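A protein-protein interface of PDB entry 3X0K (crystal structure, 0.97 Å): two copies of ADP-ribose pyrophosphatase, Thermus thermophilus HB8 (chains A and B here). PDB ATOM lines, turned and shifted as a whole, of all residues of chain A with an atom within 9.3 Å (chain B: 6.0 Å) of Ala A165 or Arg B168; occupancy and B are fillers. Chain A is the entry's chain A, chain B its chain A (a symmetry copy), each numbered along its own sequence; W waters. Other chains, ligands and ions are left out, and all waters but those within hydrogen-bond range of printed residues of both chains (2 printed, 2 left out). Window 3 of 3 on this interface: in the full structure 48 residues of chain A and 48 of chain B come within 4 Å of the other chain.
Water W1 lies within hydrogen-bond range of NH2 of Arg B168 (3.1 Å) and O of Ala A165 (3.3 Å). Water W2 lies within hydrogen-bond range of NH2 of Arg A168 (3.1 Å) and O of Ala B165 (3.3 Å).
Val A158 touches Leu B161. CB of Leu A161 touches CB of Leu B161 (3.7 Å). Leu A161 touches Ala B165 (O to CB, 3.98 Å). Phe B166 touches Leu A161 (CE1 to CD2, 3.97 Å). His A164 touches Ala B165. Phe B166 touches His A164. His B164 touches Ala A165 (CB to CB, 3.7 Å). Ala B165 touches Ala A165 (CA to CA, 3.7 Å). CE1 of Phe A166 touches CD2 of Leu B161, at 3.98 Å. Arg A168 touches Ala B165.
Of the 16 printed residues of chain A, 6 touch a printed residue of chain B. Printed residues of chain A that touch a printed residue of chain B: Val A158, Leu A161, His A164, Ala A165, Phe A166 and Arg A168. Hydrophobic or aromatic side chains of chain A within 4 Å of the printed part of chain B: Val A158, Leu A161, His A164, Ala A165 and Phe A166. Of the 8 printed residues of chain B, 5 touch a printed residue of chain A. Hydrophobic or aromatic side chains of chain B that line the printed part of chain A: Leu B161, His B164, Ala B165 and Phe B166. Among the printed residues, 13 pairs touch across the chains. Among the printed residues, no Asp or Glu carboxylate lies within 4 Å of a Lys or Arg side-chain nitrogen of the other chain.
Of the printed residues of chain B, Ala A165 touches Leu B161, His B164, Ala B165 and Arg B168. Of chain A, only Ala A165 (3.7 Å) comes within 4 Å of Arg B168. Printed residues of chain B within 4 Å of Phe A166: Leu B161 and His B164. Printed residues of chain A within 4 Å of Ala B165: Leu A161 (3.98 Å), His A164 (3.7 Å), Ala A165 (3.7 Å) and Arg A168 (3.7 Å). Leu A157 touches none of the printed residues of chain B. Glu A139 touches none of the printed residues of chain B. The nearest printed residue of chain B that does not touch Ala A165 is Phe B166 (6.1 Å). The nearest residue of chain A that does not touch Arg B168 is Phe A166 (4.7 Å).
NH2 of Arg A168 lies within hydrogen-bond range of O of His A164, 3.1 Å away. The backbone carbonyl oxygen (O) of His B164 sits at hydrogen-bond distance from the guanidinium group (NH2) of Arg B168, at 3.1 Å. The backbone carbonyl oxygen (O) of Val A160 lies within hydrogen-bond range of a ring nitrogen (ND1) of His A164.
Leu A161 touches Phe B166, and with the chains exchanged Phe A166 touches Leu B161. His A164 touches Ala B165, and with the chains exchanged Ala A165 touches His B164. His A164 touches Phe B166, and with the chains exchanged Phe A166 touches His B164. Ala A165 touches its own counterpart, Ala B165. Positions printed for both chains: 139, 161, 163, 164, 165, 166, 167 and 168.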
ATOM      1  N   MET A  47      17.493 -21.181  -0.514  1.00  0.00           N
ATOM      2  CA  MET A  47      17.733 -19.930  -1.190  1.00  0.00           C
ATOM      3  C   MET A  47      16.430 -19.182  -1.367  1.00  0.00           C
ATOM      4  O   MET A  47      15.356 -19.743  -1.538  1.00  0.00           O
ATOM      5  CB  MET A  47      18.389 -20.228  -2.561  1.00  0.00           C
ATOM      6  CG  MET A  47      18.647 -18.984  -3.430  1.00  0.00           C
ATOM      7  SD  MET A  47      19.900 -19.342  -4.705  1.00  0.00           S
ATOM      8  CE  MET A  47      21.308 -19.528  -3.695  1.00  0.00           C
ATOM      9  N   PHE A  97      29.625  -9.849  -8.396  1.00  0.00           N
ATOM     10  CA  PHE A  97      30.053  -9.797  -9.790  1.00  0.00           C
ATOM     11  C   PHE A  97      28.889  -9.213 -10.585  1.00  0.00           C
ATOM     12  O   PHE A  97      27.785  -9.023 -10.041  1.00  0.00           O
ATOM     13  CB  PHE A  97      30.476 -11.178 -10.324  1.00  0.00           C
ATOM     14  CG  PHE A  97      29.641 -12.356  -9.854  1.00  0.00           C
ATOM     15  CD1 PHE A  97      30.253 -13.403  -9.154  1.00  0.00           C
ATOM     16  CD2 PHE A  97      28.272 -12.428 -10.124  1.00  0.00           C
ATOM     17  CE1 PHE A  97      29.502 -14.462  -8.709  1.00  0.00           C
ATOM     18  CE2 PHE A  97      27.521 -13.472  -9.664  1.00  0.00           C
ATOM     19  CZ  PHE A  97      28.124 -14.547  -8.935  1.00  0.00           C
ATOM     20  N   PRO A 138      18.479 -24.937  -3.108  1.00  0.00           N
ATOM     21  CA  PRO A 138      18.928 -24.831  -4.478  1.00  0.00           C
ATOM     22  C   PRO A 138      19.026 -26.199  -5.181  1.00  0.00           C
ATOM     23  O   PRO A 138      18.878 -26.246  -6.393  1.00  0.00           O
ATOM     24  CB  PRO A 138      20.328 -24.201  -4.384  1.00  0.00           C
ATOM     25  CG  PRO A 138      20.238 -23.384  -3.138  1.00  0.00           C
ATOM     26  CD  PRO A 138      19.385 -24.216  -2.176  1.00  0.00           C
ATOM     27  N   GLU A 139      19.330 -27.244  -4.428  1.00  0.00           N
ATOM     28  CA  GLU A 139      19.427 -28.570  -5.047  1.00  0.00           C
ATOM     29  C   GLU A 139      18.069 -28.954  -5.594  1.00  0.00           C
ATOM     30  O   GLU A 139      17.969 -29.597  -6.643  1.00  0.00           O
ATOM     31  CB  GLU A 139      19.829 -29.569  -3.916  1.00  0.00           C
ATOM     32  CG  GLU A 139      21.201 -29.337  -3.393  1.00  0.00           C
ATOM     33  CD  GLU A 139      21.343 -28.423  -2.216  1.00  0.00           C
ATOM     34  OE1 GLU A 139      20.390 -27.649  -1.904  1.00  0.00           O
ATOM     35  OE2 GLU A 139      22.424 -28.452  -1.589  1.00  0.00           O
ATOM     36  N   LEU A 157      19.212 -18.924 -12.064  1.00  0.00           N
ATOM     37  CA  LEU A 157      20.259 -19.893 -12.373  1.00  0.00           C
ATOM     38  C   LEU A 157      21.582 -19.473 -11.795  1.00  0.00           C
ATOM     39  O   LEU A 157      22.312 -20.322 -11.242  1.00  0.00           O
ATOM     40  CB  LEU A 157      20.355 -20.050 -13.920  1.00  0.00           C
ATOM     41  CG  LEU A 157      21.459 -20.988 -14.377  1.00  0.00           C
ATOM     42  CD1 LEU A 157      21.222 -22.417 -13.888  1.00  0.00           C
ATOM     43  CD2 LEU A 157      21.528 -20.958 -15.917  1.00  0.00           C
ATOM     44  N   VAL A 158      21.931 -18.199 -11.906  1.00  0.00           N
ATOM     45  CA  VAL A 158      23.187 -17.716 -11.296  1.00  0.00           C
ATOM     46  C   VAL A 158      23.168 -17.968  -9.815  1.00  0.00           C
ATOM     47  O   VAL A 158      24.171 -18.409  -9.255  1.00  0.00           O
ATOM     48  CB  VAL A 158      23.369 -16.214 -11.651  1.00  0.00           C
ATOM     49  CG1 VAL A 158      24.396 -15.557 -10.732  1.00  0.00           C
ATOM     50  CG2 VAL A 158      23.764 -16.067 -13.116  1.00  0.00           C
ATOM     51  N   GLY A 159      22.035 -17.707  -9.127  1.00  0.00           N
ATOM     52  CA  GLY A 159      21.995 -18.000  -7.696  1.00  0.00           C
ATOM     53  C   GLY A 159      22.259 -19.474  -7.407  1.00  0.00           C
ATOM     54  O   GLY A 159      23.012 -19.823  -6.519  1.00  0.00           O
ATOM     55  N   VAL A 160      21.584 -20.356  -8.141  1.00  0.00           N
ATOM     56  CA  VAL A 160      21.760 -21.784  -7.925  1.00  0.00           C
ATOM     57  C   VAL A 160      23.174 -22.225  -8.168  1.00  0.00           C
ATOM     58  O   VAL A 160      23.738 -23.016  -7.397  1.00  0.00           O
ATOM     59  CB  VAL A 160      20.755 -22.573  -8.823  1.00  0.00           C
ATOM     60  CG1 VAL A 160      21.074 -24.029  -8.897  1.00  0.00           C
ATOM     61  CG2 VAL A 160      19.339 -22.360  -8.322  1.00  0.00           C
ATOM     62  N   LEU A 161      23.787 -21.754  -9.259  1.00  0.00           N
ATOM     63  CA  LEU A 161      25.160 -22.166  -9.557  1.00  0.00           C
ATOM     64  C   LEU A 161      26.156 -21.611  -8.552  1.00  0.00           C
ATOM     65  O   LEU A 161      27.060 -22.294  -8.127  1.00  0.00           O
ATOM     66  CB  LEU A 161      25.536 -21.771 -10.990  1.00  0.00           C
ATOM     67  CG  LEU A 161      24.742 -22.461 -12.085  1.00  0.00           C
ATOM     68  CD1 LEU A 161      25.144 -21.932 -13.444  1.00  0.00           C
ATOM     69  CD2 LEU A 161      24.877 -23.977 -12.041  1.00  0.00           C
ATOM     70  N   TYR A 162      25.955 -20.321  -8.169  1.00  0.00           N
ATOM     71  CA  TYR A 162      26.847 -19.735  -7.169  1.00  0.00           C
ATOM     72  C   TYR A 162      26.789 -20.532  -5.879  1.00  0.00           C
ATOM     73  O   TYR A 162      27.805 -20.781  -5.250  1.00  0.00           O
ATOM     74  CB  TYR A 162      26.392 -18.254  -6.932  1.00  0.00           C
ATOM     75  CG  TYR A 162      27.342 -17.609  -5.926  1.00  0.00           C
ATOM     76  CD1 TYR A 162      28.541 -17.052  -6.387  1.00  0.00           C
ATOM     77  CD2 TYR A 162      27.048 -17.563  -4.572  1.00  0.00           C
ATOM     78  CE1 TYR A 162      29.431 -16.443  -5.478  1.00  0.00           C
ATOM     79  CE2 TYR A 162      27.917 -17.002  -3.676  1.00  0.00           C
ATOM     80  CZ  TYR A 162      29.084 -16.449  -4.131  1.00  0.00           C
ATOM     81  OH  TYR A 162      29.991 -15.906  -3.251  1.00  0.00           O
ATOM     82  N   TYR A 163      25.578 -20.898  -5.442  1.00  0.00           N
ATOM     83  CA  TYR A 163      25.473 -21.707  -4.205  1.00  0.00           C
ATOM     84  C   TYR A 163      26.279 -22.997  -4.339  1.00  0.00           C
ATOM     85  O   TYR A 163      27.008 -23.367  -3.438  1.00  0.00           O
ATOM     86  CB  TYR A 163      23.990 -22.007  -3.955  1.00  0.00           C
ATOM     87  CG  TYR A 163      23.799 -23.183  -3.010  1.00  0.00           C
ATOM     88  CD1 TYR A 163      23.774 -22.986  -1.599  1.00  0.00           C
ATOM     89  CD2 TYR A 163      23.614 -24.486  -3.447  1.00  0.00           C
ATOM     90  CE1 TYR A 163      23.595 -24.032  -0.734  1.00  0.00           C
ATOM     91  CE2 TYR A 163      23.451 -25.561  -2.603  1.00  0.00           C
ATOM     92  CZ  TYR A 163      23.421 -25.311  -1.239  1.00  0.00           C
ATOM     93  OH  TYR A 163      23.273 -26.378  -0.368  1.00  0.00           O
ATOM     94  N   HIS A 164      26.101 -23.700  -5.466  1.00  0.00           N
ATOM     95  CA  HIS A 164      26.753 -24.999  -5.560  1.00  0.00           C
ATOM     96  C   HIS A 164      28.278 -24.803  -5.631  1.00  0.00           C
ATOM     97  O   HIS A 164      29.006 -25.667  -5.193  1.00  0.00           O
ATOM     98  CB  HIS A 164      26.245 -25.761  -6.774  1.00  0.00           C
ATOM     99  CG  HIS A 164      24.927 -26.399  -6.620  1.00  0.00           C
ATOM    100  ND1 HIS A 164      23.716 -25.777  -6.873  1.00  0.00           N
ATOM    101  CD2 HIS A 164      24.585 -27.690  -6.245  1.00  0.00           C
ATOM    102  CE1 HIS A 164      22.721 -26.658  -6.641  1.00  0.00           C
ATOM    103  NE2 HIS A 164      23.231 -27.826  -6.277  1.00  0.00           N
ATOM    104  N   ALA A 165      28.737 -23.704  -6.225  1.00  0.00           N
ATOM    105  CA  ALA A 165      30.159 -23.458  -6.307  1.00  0.00           C
ATOM    106  C   ALA A 165      30.768 -23.050  -4.989  1.00  0.00           C
ATOM    107  O   ALA A 165      31.894 -23.480  -4.673  1.00  0.00           O
ATOM    108  CB  ALA A 165      30.406 -22.321  -7.317  1.00  0.00           C
ATOM    109  N   PHE A 166      30.100 -22.206  -4.204  1.00  0.00           N
ATOM    110  CA  PHE A 166      30.775 -21.528  -3.127  1.00  0.00           C
ATOM    111  C   PHE A 166      30.084 -21.546  -1.774  1.00  0.00           C
ATOM    112  O   PHE A 166      30.744 -21.112  -0.823  1.00  0.00           O
ATOM    113  CB  PHE A 166      31.004 -20.028  -3.517  1.00  0.00           C
ATOM    114  CG  PHE A 166      31.798 -19.866  -4.779  1.00  0.00           C
ATOM    115  CD1 PHE A 166      31.282 -19.267  -5.933  1.00  0.00           C
ATOM    116  CD2 PHE A 166      33.122 -20.284  -4.847  1.00  0.00           C
ATOM    117  CE1 PHE A 166      32.044 -19.128  -7.068  1.00  0.00           C
ATOM    118  CE2 PHE A 166      33.904 -20.164  -5.989  1.00  0.00           C
ATOM    119  CZ  PHE A 166      33.360 -19.541  -7.124  1.00  0.00           C
ATOM    120  N   LEU A 167      28.849 -22.003  -1.662  1.00  0.00           N
ATOM    121  CA  LEU A 167      28.125 -21.838  -0.388  1.00  0.00           C
ATOM    122  C   LEU A 167      27.784 -23.161   0.273  1.00  0.00           C
ATOM    123  O   LEU A 167      27.040 -23.139   1.257  1.00  0.00           O
ATOM    124  CB  LEU A 167      26.842 -21.058  -0.615  1.00  0.00           C
ATOM    125  CG  LEU A 167      26.985 -19.657  -1.124  1.00  0.00           C
ATOM    126  CD1 LEU A 167      25.629 -18.977  -1.283  1.00  0.00           C
ATOM    127  CD2 LEU A 167      27.844 -18.793  -0.182  1.00  0.00           C
ATOM    128  N   ARG A 168      28.343 -24.250  -0.207  1.00  0.00           N
ATOM    129  CA  ARG A 168      28.021 -25.514   0.499  1.00  0.00           C
ATOM    130  C   ARG A 168      29.064 -25.752   1.636  1.00  0.00           C
ATOM    131  O   ARG A 168      28.460 -26.542   2.398  1.00  0.00           O
ATOM    132  CB  ARG A 168      27.898 -26.721  -0.468  1.00  0.00           C
ATOM    133  CG  ARG A 168      26.704 -26.467  -1.473  1.00  0.00           C
ATOM    134  CD  ARG A 168      26.504 -27.771  -2.232  1.00  0.00           C
ATOM    135  NE  ARG A 168      27.534 -27.813  -3.294  1.00  0.00           N
ATOM    136  CZ  ARG A 168      27.673 -28.787  -4.209  1.00  0.00           C
ATOM    137  NH1 ARG A 168      26.793 -29.785  -4.108  1.00  0.00           N
ATOM    138  NH2 ARG A 168      28.626 -28.707  -5.104  1.00  0.00           N
ATOM    139  N   GLU B 139      39.174 -19.874 -13.124  1.00  0.00           N
ATOM    140  CA  GLU B 139      39.572 -19.168 -11.902  1.00  0.00           C
ATOM    141  C   GLU B 139      40.170 -17.830 -12.283  1.00  0.00           C
ATOM    142  O   GLU B 139      39.987 -16.834 -11.579  1.00  0.00           O
ATOM    143  CB  GLU B 139      40.665 -20.043 -11.208  1.00  0.00           C
ATOM    144  CG  GLU B 139      40.139 -21.337 -10.698  1.00  0.00           C
ATOM    145  CD  GLU B 139      40.211 -22.517 -11.616  1.00  0.00           C
ATOM    146  OE1 GLU B 139      40.404 -22.339 -12.855  1.00  0.00           O
ATOM    147  OE2 GLU B 139      40.057 -23.650 -11.111  1.00  0.00           O
ATOM    148  N   LEU B 161      30.619 -20.228 -13.291  1.00  0.00           N
ATOM    149  CA  LEU B 161      29.998 -20.758 -12.076  1.00  0.00           C
ATOM    150  C   LEU B 161      29.755 -22.255 -12.164  1.00  0.00           C
ATOM    151  O   LEU B 161      29.973 -22.980 -11.220  1.00  0.00           O
ATOM    152  CB  LEU B 161      28.702 -20.001 -11.766  1.00  0.00           C
ATOM    153  CG  LEU B 161      28.872 -18.529 -11.431  1.00  0.00           C
ATOM    154  CD1 LEU B 161      27.525 -17.873 -11.226  1.00  0.00           C
ATOM    155  CD2 LEU B 161      29.766 -18.303 -10.220  1.00  0.00           C
ATOM    156  N   TYR B 163      31.476 -24.403 -13.879  1.00  0.00           N
ATOM    157  CA  TYR B 163      32.773 -25.087 -13.663  1.00  0.00           C
ATOM    158  C   TYR B 163      33.080 -25.193 -12.170  1.00  0.00           C
ATOM    159  O   TYR B 163      33.481 -26.238 -11.693  1.00  0.00           O
ATOM    160  CB  TYR B 163      33.861 -24.292 -14.394  1.00  0.00           C
ATOM    161  CG  TYR B 163      35.251 -24.621 -13.875  1.00  0.00           C
ATOM    162  CD1 TYR B 163      35.991 -25.712 -14.415  1.00  0.00           C
ATOM    163  CD2 TYR B 163      35.887 -23.882 -12.888  1.00  0.00           C
ATOM    164  CE1 TYR B 163      37.248 -26.017 -13.965  1.00  0.00           C
ATOM    165  CE2 TYR B 163      37.142 -24.175 -12.401  1.00  0.00           C
ATOM    166  CZ  TYR B 163      37.822 -25.240 -12.972  1.00  0.00           C
ATOM    167  OH  TYR B 163      39.080 -25.563 -12.489  1.00  0.00           O
ATOM    168  N   HIS B 164      32.928 -24.075 -11.447  1.00  0.00           N
ATOM    169  CA  HIS B 164      33.342 -24.113 -10.051  1.00  0.00           C
ATOM    170  C   HIS B 164      32.405 -25.046  -9.263  1.00  0.00           C
ATOM    171  O   HIS B 164      32.833 -25.630  -8.292  1.00  0.00           O
ATOM    172  CB  HIS B 164      33.340 -22.712  -9.459  1.00  0.00           C
ATOM    173  CG  HIS B 164      34.496 -21.870  -9.812  1.00  0.00           C
ATOM    174  ND1 HIS B 164      34.574 -21.072 -10.940  1.00  0.00           N
ATOM    175  CD2 HIS B 164      35.691 -21.650  -9.145  1.00  0.00           C
ATOM    176  CE1 HIS B 164      35.762 -20.434 -10.937  1.00  0.00           C
ATOM    177  NE2 HIS B 164      36.443 -20.759  -9.848  1.00  0.00           N
ATOM    178  N   ALA B 165      31.136 -25.130  -9.656  1.00  0.00           N
ATOM    179  CA  ALA B 165      30.214 -26.002  -8.966  1.00  0.00           C
ATOM    180  C   ALA B 165      30.446 -27.463  -9.258  1.00  0.00           C
ATOM    181  O   ALA B 165      30.329 -28.299  -8.342  1.00  0.00           O
ATOM    182  CB  ALA B 165      28.779 -25.651  -9.404  1.00  0.00           C
ATOM    183  N   PHE B 166      30.734 -27.833 -10.505  1.00  0.00           N
ATOM    184  CA  PHE B 166      30.620 -29.214 -10.898  1.00  0.00           C
ATOM    185  C   PHE B 166      31.796 -29.803 -11.660  1.00  0.00           C
ATOM    186  O   PHE B 166      31.764 -31.024 -11.845  1.00  0.00           O
ATOM    187  CB  PHE B 166      29.344 -29.401 -11.786  1.00  0.00           C
ATOM    188  CG  PHE B 166      28.083 -28.977 -11.094  1.00  0.00           C
ATOM    189  CD1 PHE B 166      27.281 -27.924 -11.547  1.00  0.00           C
ATOM    190  CD2 PHE B 166      27.628 -29.649  -9.965  1.00  0.00           C
ATOM    191  CE1 PHE B 166      26.126 -27.571 -10.891  1.00  0.00           C
ATOM    192  CE2 PHE B 166      26.470 -29.299  -9.281  1.00  0.00           C
ATOM    193  CZ  PHE B 166      25.679 -28.249  -9.774  1.00  0.00           C
ATOM    194  N   LEU B 167      32.772 -29.021 -12.088  1.00  0.00           N
ATOM    195  CA  LEU B 167      33.803 -29.571 -12.987  1.00  0.00           C
ATOM    196  C   LEU B 167      35.190 -29.560 -12.373  1.00  0.00           C
ATOM    197  O   LEU B 167      36.145 -29.846 -13.099  1.00  0.00           O
ATOM    198  CB  LEU B 167      33.835 -28.785 -14.286  1.00  0.00           C
ATOM    199  CG  LEU B 167      32.591 -28.805 -15.119  1.00  0.00           C
ATOM    200  CD1 LEU B 167      32.764 -28.001 -16.405  1.00  0.00           C
ATOM    201  CD2 LEU B 167      32.189 -30.240 -15.505  1.00  0.00           C
ATOM    202  N   ARG B 168      35.290 -29.297 -11.088  1.00  0.00           N
ATOM    203  CA  ARG B 168      36.659 -29.345 -10.517  1.00  0.00           C
ATOM    204  C   ARG B 168      36.960 -30.791 -10.015  1.00  0.00           C
ATOM    205  O   ARG B 168      38.212 -30.814  -9.986  1.00  0.00           O
ATOM    206  CB  ARG B 168      36.885 -28.268  -9.424  1.00  0.00           C
ATOM    207  CG  ARG B 168      36.730 -26.829 -10.065  1.00  0.00           C
ATOM    208  CD  ARG B 168      37.181 -25.841  -9.001  1.00  0.00           C
ATOM    209  NE  ARG B 168      36.046 -25.666  -8.067  1.00  0.00           N
ATOM    210  CZ  ARG B 168      36.026 -24.843  -7.005  1.00  0.00           C
ATOM    211  NH1 ARG B 168      37.150 -24.150  -6.809  1.00  0.00           N
ATOM    212  NH2 ARG B 168      34.957 -24.776  -6.253  1.00  0.00           N
HETATM  213  O   HOH W   1      35.062 -23.229  -3.619  1.00  0.00           O
HETATM  214  O   HOH W   2      29.201 -31.106  -6.908  1.00  0.00           O
